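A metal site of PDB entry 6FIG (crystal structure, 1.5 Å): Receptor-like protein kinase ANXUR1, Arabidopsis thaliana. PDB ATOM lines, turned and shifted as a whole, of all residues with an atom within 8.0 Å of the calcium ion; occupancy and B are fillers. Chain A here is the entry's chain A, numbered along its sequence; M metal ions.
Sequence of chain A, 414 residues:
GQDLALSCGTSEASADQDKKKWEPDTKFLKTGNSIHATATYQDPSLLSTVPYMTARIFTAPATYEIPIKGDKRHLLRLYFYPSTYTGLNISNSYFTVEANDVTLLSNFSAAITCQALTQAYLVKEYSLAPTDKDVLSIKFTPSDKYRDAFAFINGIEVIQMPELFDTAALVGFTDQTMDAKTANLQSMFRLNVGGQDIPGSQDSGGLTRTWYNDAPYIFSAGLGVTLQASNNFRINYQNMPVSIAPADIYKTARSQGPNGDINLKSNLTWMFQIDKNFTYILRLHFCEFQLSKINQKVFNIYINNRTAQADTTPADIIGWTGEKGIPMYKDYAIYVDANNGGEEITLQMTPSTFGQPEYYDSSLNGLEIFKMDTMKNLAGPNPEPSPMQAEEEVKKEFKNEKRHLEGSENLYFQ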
ATOM      1  N   LEU A 191      23.513 -12.537  -5.167  1.00  0.00           N
ATOM      2  CA  LEU A 191      23.749 -13.204  -3.898  1.00  0.00           C
ATOM      3  C   LEU A 191      22.510 -13.802  -3.269  1.00  0.00           C
ATOM      4  O   LEU A 191      21.450 -13.168  -3.249  1.00  0.00           O
ATOM      5  CB  LEU A 191      24.366 -12.244  -2.867  1.00  0.00           C
ATOM      6  CG  LEU A 191      25.591 -11.460  -3.294  1.00  0.00           C
ATOM      7  CD1 LEU A 191      26.030 -10.542  -2.172  1.00  0.00           C
ATOM      8  CD2 LEU A 191      26.736 -12.371  -3.736  1.00  0.00           C
ATOM      9  N   ASN A 192      22.655 -15.018  -2.768  1.00  0.00           N
ATOM     10  CA  ASN A 192      21.700 -15.587  -1.821  1.00  0.00           C
ATOM     11  C   ASN A 192      22.180 -15.193  -0.433  1.00  0.00           C
ATOM     12  O   ASN A 192      23.110 -15.791   0.103  1.00  0.00           O
ATOM     13  CB  ASN A 192      21.660 -17.111  -1.948  1.00  0.00           C
ATOM     14  CG  ASN A 192      20.628 -17.747  -1.051  1.00  0.00           C
ATOM     15  OD1 ASN A 192      19.799 -17.023  -0.481  1.00  0.00           O
ATOM     16  ND2 ASN A 192      20.664 -19.064  -0.915  1.00  0.00           N
ATOM     17  N   VAL A 193      21.526 -14.174   0.122  1.00  0.00           N
ATOM     18  CA  VAL A 193      21.927 -13.633   1.427  1.00  0.00           C
ATOM     19  C   VAL A 193      21.518 -14.609   2.539  1.00  0.00           C
ATOM     20  O   VAL A 193      20.356 -15.004   2.660  1.00  0.00           O
ATOM     21  CB  VAL A 193      21.384 -12.203   1.622  1.00  0.00           C
ATOM     22  CG1 VAL A 193      21.735 -11.687   3.019  1.00  0.00           C
ATOM     23  CG2 VAL A 193      21.969 -11.273   0.582  1.00  0.00           C
ATOM     24  N   GLY A 194      22.509 -15.020   3.311  1.00  0.00           N
ATOM     25  CA  GLY A 194      22.312 -15.948   4.418  1.00  0.00           C
ATOM     26  C   GLY A 194      22.155 -17.395   4.037  1.00  0.00           C
ATOM     27  O   GLY A 194      21.898 -18.221   4.901  1.00  0.00           O
ATOM     28  N   GLY A 195      22.309 -17.735   2.749  1.00  0.00           N
ATOM     29  CA  GLY A 195      22.093 -19.111   2.291  1.00  0.00           C
ATOM     30  C   GLY A 195      23.237 -19.619   1.455  1.00  0.00           C
ATOM     31  O   GLY A 195      24.156 -18.870   1.120  1.00  0.00           O
ATOM     32  N   GLN A 196      23.145 -20.890   1.101  1.00  0.00           N
ATOM     33  CA  GLN A 196      24.172 -21.551   0.296  1.00  0.00           C
ATOM     34  C   GLN A 196      24.057 -21.129  -1.163  1.00  0.00           C
ATOM     35  O   GLN A 196      23.012 -20.667  -1.620  1.00  0.00           O
ATOM     36  CB  GLN A 196      24.035 -23.081   0.389  1.00  0.00           C
ATOM     37  CG  GLN A 196      24.291 -23.633   1.784  1.00  0.00           C
ATOM     38  CD  GLN A 196      24.123 -25.142   1.875  1.00  0.00           C
ATOM     39  OE1 GLN A 196      23.289 -25.643   2.625  1.00  0.00           O
ATOM     40  NE2 GLN A 196      24.934 -25.870   1.113  1.00  0.00           N
ATOM     41  N   ILE A 198      23.211 -21.194  -4.846  1.00  0.00           N
ATOM     42  CA  ILE A 198      22.184 -21.822  -5.646  1.00  0.00           C
ATOM     43  C   ILE A 198      22.745 -21.963  -7.072  1.00  0.00           C
ATOM     44  O   ILE A 198      22.977 -20.940  -7.715  1.00  0.00           O
ATOM     45  CB  ILE A 198      20.911 -20.953  -5.711  1.00  0.00           C
ATOM     46  CG1 ILE A 198      20.365 -20.688  -4.312  1.00  0.00           C
ATOM     47  CG2 ILE A 198      19.848 -21.650  -6.562  1.00  0.00           C
ATOM     48  CD1 ILE A 198      19.208 -19.705  -4.277  1.00  0.00           C
ATOM     49  N   TRP A 211      23.243 -18.046  -7.823  1.00  0.00           N
ATOM     50  CA  TRP A 211      23.105 -17.119  -6.677  1.00  0.00           C
ATOM     51  C   TRP A 211      24.148 -17.519  -5.628  1.00  0.00           C
ATOM     52  O   TRP A 211      24.126 -18.633  -5.116  1.00  0.00           O
ATOM     53  CB  TRP A 211      21.708 -17.159  -6.102  1.00  0.00           C
ATOM     54  CG  TRP A 211      20.614 -16.873  -7.078  1.00  0.00           C
ATOM     55  CD1 TRP A 211      20.161 -17.699  -8.089  1.00  0.00           C
ATOM     56  CD2 TRP A 211      19.841 -15.656  -7.176  1.00  0.00           C
ATOM     57  NE1 TRP A 211      19.130 -17.069  -8.773  1.00  0.00           N
ATOM     58  CE2 TRP A 211      18.932 -15.824  -8.242  1.00  0.00           C
ATOM     59  CE3 TRP A 211      19.820 -14.461  -6.441  1.00  0.00           C
ATOM     60  CZ2 TRP A 211      18.050 -14.830  -8.605  1.00  0.00           C
ATOM     61  CZ3 TRP A 211      18.928 -13.487  -6.799  1.00  0.00           C
ATOM     62  CH2 TRP A 211      18.050 -13.675  -7.862  1.00  0.00           C
ATOM     63  N   TYR A 212      25.080 -16.635  -5.326  1.00  0.00           N
ATOM     64  CA  TYR A 212      26.234 -16.995  -4.479  1.00  0.00           C
ATOM     65  C   TYR A 212      26.024 -16.579  -3.030  1.00  0.00           C
ATOM     66  O   TYR A 212      25.391 -15.536  -2.750  1.00  0.00           O
ATOM     67  CB  TYR A 212      27.480 -16.317  -4.999  1.00  0.00           C
ATOM     68  CG  TYR A 212      27.874 -16.745  -6.391  1.00  0.00           C
ATOM     69  CD1 TYR A 212      28.706 -17.836  -6.565  1.00  0.00           C
ATOM     70  CD2 TYR A 212      27.411 -16.069  -7.520  1.00  0.00           C
ATOM     71  CE1 TYR A 212      29.089 -18.239  -7.853  1.00  0.00           C
ATOM     72  CE2 TYR A 212      27.778 -16.461  -8.797  1.00  0.00           C
ATOM     73  CZ  TYR A 212      28.612 -17.545  -8.959  1.00  0.00           C
ATOM     74  OH  TYR A 212      28.964 -17.925 -10.225  1.00  0.00           O
ATOM     75  N   ASN A 213      26.585 -17.358  -2.115  1.00  0.00           N
ATOM     76  CA  ASN A 213      26.556 -16.964  -0.715  1.00  0.00           C
ATOM     77  C   ASN A 213      27.191 -15.576  -0.534  1.00  0.00           C
ATOM     78  O   ASN A 213      28.157 -15.222  -1.225  1.00  0.00           O
ATOM     79  CB  ASN A 213      27.240 -18.005   0.150  1.00  0.00           C
ATOM     80  CG  ASN A 213      27.293 -17.580   1.606  1.00  0.00           C
ATOM     81  OD1 ASN A 213      28.321 -17.110   2.059  1.00  0.00           O
ATOM     82  ND2 ASN A 213      26.184 -17.712   2.333  1.00  0.00           N
ATOM     83  N   ASP A 214      26.602 -14.782   0.373  1.00  0.00           N
ATOM     84  CA  ASP A 214      27.010 -13.382   0.561  1.00  0.00           C
ATOM     85  C   ASP A 214      28.166 -13.145   1.527  1.00  0.00           C
ATOM     86  O   ASP A 214      28.683 -12.032   1.589  1.00  0.00           O
ATOM     87  CB  ASP A 214      25.820 -12.541   1.004  1.00  0.00           C
ATOM     88  CG  ASP A 214      25.389 -12.850   2.412  1.00  0.00           C
ATOM     89  OD1 ASP A 214      25.207 -14.056   2.711  1.00  0.00           O
ATOM     90  OD2 ASP A 214      25.249 -11.899   3.224  1.00  0.00           O
ATOM     91  N   LEU A 227      19.481 -17.091   9.095  1.00  0.00           N
ATOM     92  CA  LEU A 227      18.193 -17.661   9.409  1.00  0.00           C
ATOM     93  C   LEU A 227      17.752 -18.558   8.264  1.00  0.00           C
ATOM     94  O   LEU A 227      18.044 -18.286   7.103  1.00  0.00           O
ATOM     95  CB  LEU A 227      17.147 -16.546   9.581  1.00  0.00           C
ATOM     96  CG  LEU A 227      17.460 -15.410  10.560  1.00  0.00           C
ATOM     97  CD1 LEU A 227      16.467 -14.269  10.375  1.00  0.00           C
ATOM     98  CD2 LEU A 227      17.445 -15.922  11.992  1.00  0.00           C
ATOM     99  N   PRO A 246      14.450 -17.538  -7.382  1.00  0.00           N
ATOM    100  CA  PRO A 246      13.931 -18.806  -6.936  1.00  0.00           C
ATOM    101  C   PRO A 246      13.556 -18.839  -5.464  1.00  0.00           C
ATOM    102  O   PRO A 246      14.042 -18.028  -4.644  1.00  0.00           O
ATOM    103  CB  PRO A 246      15.086 -19.786  -7.221  1.00  0.00           C
ATOM    104  CG  PRO A 246      16.293 -18.952  -7.165  1.00  0.00           C
ATOM    105  CD  PRO A 246      15.892 -17.609  -7.681  1.00  0.00           C
ATOM    106  N   ALA A 247      12.675 -19.770  -5.130  1.00  0.00           N
ATOM    107  CA  ALA A 247      12.109 -19.830  -3.773  1.00  0.00           C
ATOM    108  C   ALA A 247      13.168 -19.925  -2.691  1.00  0.00           C
ATOM    109  O   ALA A 247      13.020 -19.335  -1.608  1.00  0.00           O
ATOM    110  CB  ALA A 247      11.127 -20.966  -3.649  1.00  0.00           C
ATOM    111  N   ASP A 248      14.249 -20.644  -2.983  1.00  0.00           N
ATOM    112  CA  ASP A 248      15.312 -20.820  -1.992  1.00  0.00           C
ATOM    113  C   ASP A 248      15.983 -19.529  -1.553  1.00  0.00           C
ATOM    114  O   ASP A 248      16.452 -19.472  -0.407  1.00  0.00           O
ATOM    115  CB  ASP A 248      16.317 -21.890  -2.423  1.00  0.00           C
ATOM    116  CG  ASP A 248      15.850 -23.323  -2.093  1.00  0.00           C
ATOM    117  OD1 ASP A 248      14.857 -23.544  -1.353  1.00  0.00           O
ATOM    118  OD2 ASP A 248      16.478 -24.279  -2.568  1.00  0.00           O
ATOM    119  N   ILE A 249      16.023 -18.496  -2.405  1.00  0.00           N
ATOM    120  CA  ILE A 249      16.532 -17.193  -1.990  1.00  0.00           C
ATOM    121  C   ILE A 249      15.725 -16.685  -0.788  1.00  0.00           C
ATOM    122  O   ILE A 249      16.303 -16.220   0.215  1.00  0.00           O
ATOM    123  CB  ILE A 249      16.424 -16.153  -3.140  1.00  0.00           C
ATOM    124  CG1 ILE A 249      17.413 -16.512  -4.250  1.00  0.00           C
ATOM    125  CG2 ILE A 249      16.582 -14.712  -2.652  1.00  0.00           C
ATOM    126  CD1 ILE A 249      18.864 -16.399  -3.859  1.00  0.00           C
ATOM    127  N   TYR A 250      14.415 -16.785  -0.911  1.00  0.00           N
ATOM    128  CA  TYR A 250      13.501 -16.226   0.089  1.00  0.00           C
ATOM    129  C   TYR A 250      13.419 -17.056   1.366  1.00  0.00           C
ATOM    130  O   TYR A 250      12.982 -16.531   2.397  1.00  0.00           O
ATOM    131  CB  TYR A 250      12.129 -16.007  -0.562  1.00  0.00           C
ATOM    132  CG  TYR A 250      12.206 -15.042  -1.707  1.00  0.00           C
ATOM    133  CD1 TYR A 250      12.539 -13.711  -1.498  1.00  0.00           C
ATOM    134  CD2 TYR A 250      12.002 -15.459  -3.015  1.00  0.00           C
ATOM    135  CE1 TYR A 250      12.621 -12.819  -2.543  1.00  0.00           C
ATOM    136  CE2 TYR A 250      12.073 -14.566  -4.076  1.00  0.00           C
ATOM    137  CZ  TYR A 250      12.424 -13.259  -3.845  1.00  0.00           C
ATOM    138  OH  TYR A 250      12.507 -12.359  -4.877  1.00  0.00           O
ATOM    139  N   LYS A 251      13.870 -18.309   1.327  1.00  0.00           N
ATOM    140  CA  LYS A 251      13.835 -19.185   2.510  1.00  0.00           C
ATOM    141  C   LYS A 251      15.048 -19.050   3.444  1.00  0.00           C
ATOM    142  O   LYS A 251      15.116 -19.735   4.486  1.00  0.00           O
ATOM    143  CB  LYS A 251      13.661 -20.661   2.090  1.00  0.00           C
ATOM    144  CG  LYS A 251      12.323 -20.921   1.435  1.00  0.00           C
ATOM    145  CD  LYS A 251      12.212 -22.347   0.906  1.00  0.00           C
ATOM    146  CE  LYS A 251      10.925 -22.499   0.103  1.00  0.00           C
ATOM    147  NZ  LYS A 251      10.773 -23.853  -0.540  1.00  0.00           N
ATOM    148  N   THR A 252      16.015 -18.219   3.082  1.00  0.00           N
ATOM    149  CA  THR A 252      17.126 -17.908   3.951  1.00  0.00           C
ATOM    150  C   THR A 252      17.346 -16.406   4.004  1.00  0.00           C
ATOM    151  O   THR A 252      17.082 -15.687   3.047  1.00  0.00           O
ATOM    152  CB  THR A 252      18.431 -18.563   3.514  1.00  0.00           C
ATOM    153  OG1 THR A 252      18.717 -18.174   2.171  1.00  0.00           O
ATOM    154  CG2 THR A 252      18.351 -20.097   3.629  1.00  0.00           C
ATOM    155  N   ALA A 253      17.918 -15.953   5.119  1.00  0.00           N
ATOM    156  CA  ALA A 253      18.234 -14.542   5.284  1.00  0.00           C
ATOM    157  C   ALA A 253      19.429 -14.353   6.209  1.00  0.00           C
ATOM    158  O   ALA A 253      19.791 -15.260   6.983  1.00  0.00           O
ATOM    159  CB  ALA A 253      17.015 -13.794   5.837  1.00  0.00           C
ATOM    160  N   ARG A 254      20.032 -13.192   6.109  1.00  0.00           N
ATOM    161  CA  ARG A 254      20.996 -12.744   7.107  1.00  0.00           C
ATOM    162  C   ARG A 254      20.301 -11.662   7.898  1.00  0.00           C
ATOM    163  O   ARG A 254      19.638 -10.783   7.322  1.00  0.00           O
ATOM    164  CB  ARG A 254      22.286 -12.215   6.477  1.00  0.00           C
ATOM    165  CG  ARG A 254      23.408 -11.947   7.468  1.00  0.00           C
ATOM    166  CD  ARG A 254      24.686 -11.535   6.790  1.00  0.00           C
ATOM    167  NE  ARG A 254      25.177 -12.597   5.895  1.00  0.00           N
ATOM    168  CZ  ARG A 254      25.816 -13.703   6.293  1.00  0.00           C
ATOM    169  NH1 ARG A 254      26.112 -13.917   7.574  1.00  0.00           N
ATOM    170  NH2 ARG A 254      26.199 -14.604   5.395  1.00  0.00           N
ATOM    171  N   HIS A 285      16.166  -8.280  -2.068  1.00  0.00           N
ATOM    172  CA  HIS A 285      15.118  -9.290  -1.988  1.00  0.00           C
ATOM    173  C   HIS A 285      14.776  -9.555  -0.516  1.00  0.00           C
ATOM    174  O   HIS A 285      15.681  -9.785   0.288  1.00  0.00           O
ATOM    175  CB  HIS A 285      15.597 -10.589  -2.625  1.00  0.00           C
ATOM    176  CG  HIS A 285      15.799 -10.512  -4.099  1.00  0.00           C
ATOM    177  ND1 HIS A 285      14.815 -10.817  -5.003  1.00  0.00           N
ATOM    178  CD2 HIS A 285      16.888 -10.165  -4.824  1.00  0.00           C
ATOM    179  CE1 HIS A 285      15.283 -10.667  -6.229  1.00  0.00           C
ATOM    180  NE2 HIS A 285      16.549 -10.278  -6.143  1.00  0.00           N
ATOM    181  N   PHE A 289       9.976 -14.750   7.079  1.00  0.00           N
ATOM    182  CA  PHE A 289       9.553 -16.123   7.372  1.00  0.00           C
ATOM    183  C   PHE A 289       9.550 -16.488   8.865  1.00  0.00           C
ATOM    184  O   PHE A 289       9.248 -17.635   9.223  1.00  0.00           O
ATOM    185  CB  PHE A 289      10.327 -17.147   6.532  1.00  0.00           C
ATOM    186  CG  PHE A 289      11.821 -17.070   6.676  1.00  0.00           C
ATOM    187  CD1 PHE A 289      12.607 -16.590   5.620  1.00  0.00           C
ATOM    188  CD2 PHE A 289      12.457 -17.504   7.837  1.00  0.00           C
ATOM    189  CE1 PHE A 289      13.976 -16.518   5.738  1.00  0.00           C
ATOM    190  CE2 PHE A 289      13.835 -17.419   7.963  1.00  0.00           C
ATOM    191  CZ  PHE A 289      14.599 -16.935   6.898  1.00  0.00           C
ATOM    192  N   LEU A 364      17.828  -9.381   5.340  1.00  0.00           N
ATOM    193  CA  LEU A 364      17.875  -9.333   3.895  1.00  0.00           C
ATOM    194  C   LEU A 364      17.964 -10.777   3.398  1.00  0.00           C
ATOM    195  O   LEU A 364      18.668 -11.598   3.999  1.00  0.00           O
ATOM    196  CB  LEU A 364      19.099  -8.528   3.445  1.00  0.00           C
ATOM    197  CG  LEU A 364      19.291  -8.365   1.922  1.00  0.00           C
ATOM    198  CD1 LEU A 364      18.170  -7.567   1.297  1.00  0.00           C
ATOM    199  CD2 LEU A 364      20.648  -7.712   1.664  1.00  0.00           C
ATOM    200  N   ASN A 365      17.252 -11.083   2.302  1.00  0.00           N
ATOM    201  CA  ASN A 365      17.222 -12.482   1.780  1.00  0.00           C
ATOM    202  C   ASN A 365      18.034 -12.700   0.508  1.00  0.00           C
ATOM    203  O   ASN A 365      18.506 -13.801   0.260  1.00  0.00           O
ATOM    204  CB  ASN A 365      15.786 -12.922   1.516  1.00  0.00           C
ATOM    205  CG  ASN A 365      14.884 -12.832   2.756  1.00  0.00           C
ATOM    206  OD1 ASN A 365      14.668 -11.730   3.266  1.00  0.00           O
ATOM    207  ND2 ASN A 365      14.332 -13.976   3.208  1.00  0.00           N
ATOM    208  N   GLY A 366      18.206 -11.648  -0.286  1.00  0.00           N
ATOM    209  CA  GLY A 366      18.933 -11.759  -1.543  1.00  0.00           C
ATOM    210  C   GLY A 366      19.390 -10.392  -1.991  1.00  0.00           C
ATOM    211  O   GLY A 366      18.825  -9.365  -1.553  1.00  0.00           O
ATOM    212  N   LEU A 367      20.353 -10.367  -2.904  1.00  0.00           N
ATOM    213  CA  LEU A 367      20.867  -9.103  -3.407  1.00  0.00           C
ATOM    214  C   LEU A 367      21.414  -9.252  -4.800  1.00  0.00           C
ATOM    215  O   LEU A 367      22.257 -10.103  -5.026  1.00  0.00           O
ATOM    216  CB  LEU A 367      21.976  -8.570  -2.500  1.00  0.00           C
ATOM    217  CG  LEU A 367      22.624  -7.236  -2.860  1.00  0.00           C
ATOM    218  CD1 LEU A 367      21.634  -6.064  -2.912  1.00  0.00           C
ATOM    219  CD2 LEU A 367      23.731  -6.951  -1.870  1.00  0.00           C
HETATM  220 CA    CA M   1      18.563 -15.959   1.171  1.00  0.00          CA
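The side-chain amide nitrogen (ND2) of Asn 192 sits at hydrogen-bond distance from the backbone carbonyl oxygen (O) of Gln 196, 2.9 Å away. The backbone NH of Asn 192 sits at hydrogen-bond distance from the backbone carbonyl oxygen of Tyr 212 (2.8 Å). ND2 of Asn 365 lies within hydrogen-bond range of O of Tyr 250, 3.0 Å away. The backbone NH (N) of Asn 365 lies within hydrogen-bond range of the backbone carbonyl oxygen (O) of His 285 (2.9 Å). The backbone carbonyl oxygen (O) of Ala 253 is in hydrogen-bond range of the backbone NH (N) of Leu 227 (2.8 Å).
Five residues have an atom within 4 Å of the calcium ion: Asn 192, Val 193, Ile 249, Thr 252 and Asn 365. The nearest printed residue that does not touch the calcium ion is Ala 253 (4.0003 Å).
The calcium ion is bound by OD1 of Asn 192 (2.3 Å). O of Asn 365 binds the calcium ion. The calcium ion is bound by O of Thr 252 (2.4 Å). OG1 of Thr 252 binds the calcium ion. The calcium ion is bound by O of Ile 249. O of Val 193 is bound to the calcium ion, at 2.5 Å. The calcium ion has six donor atoms within binding distance.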
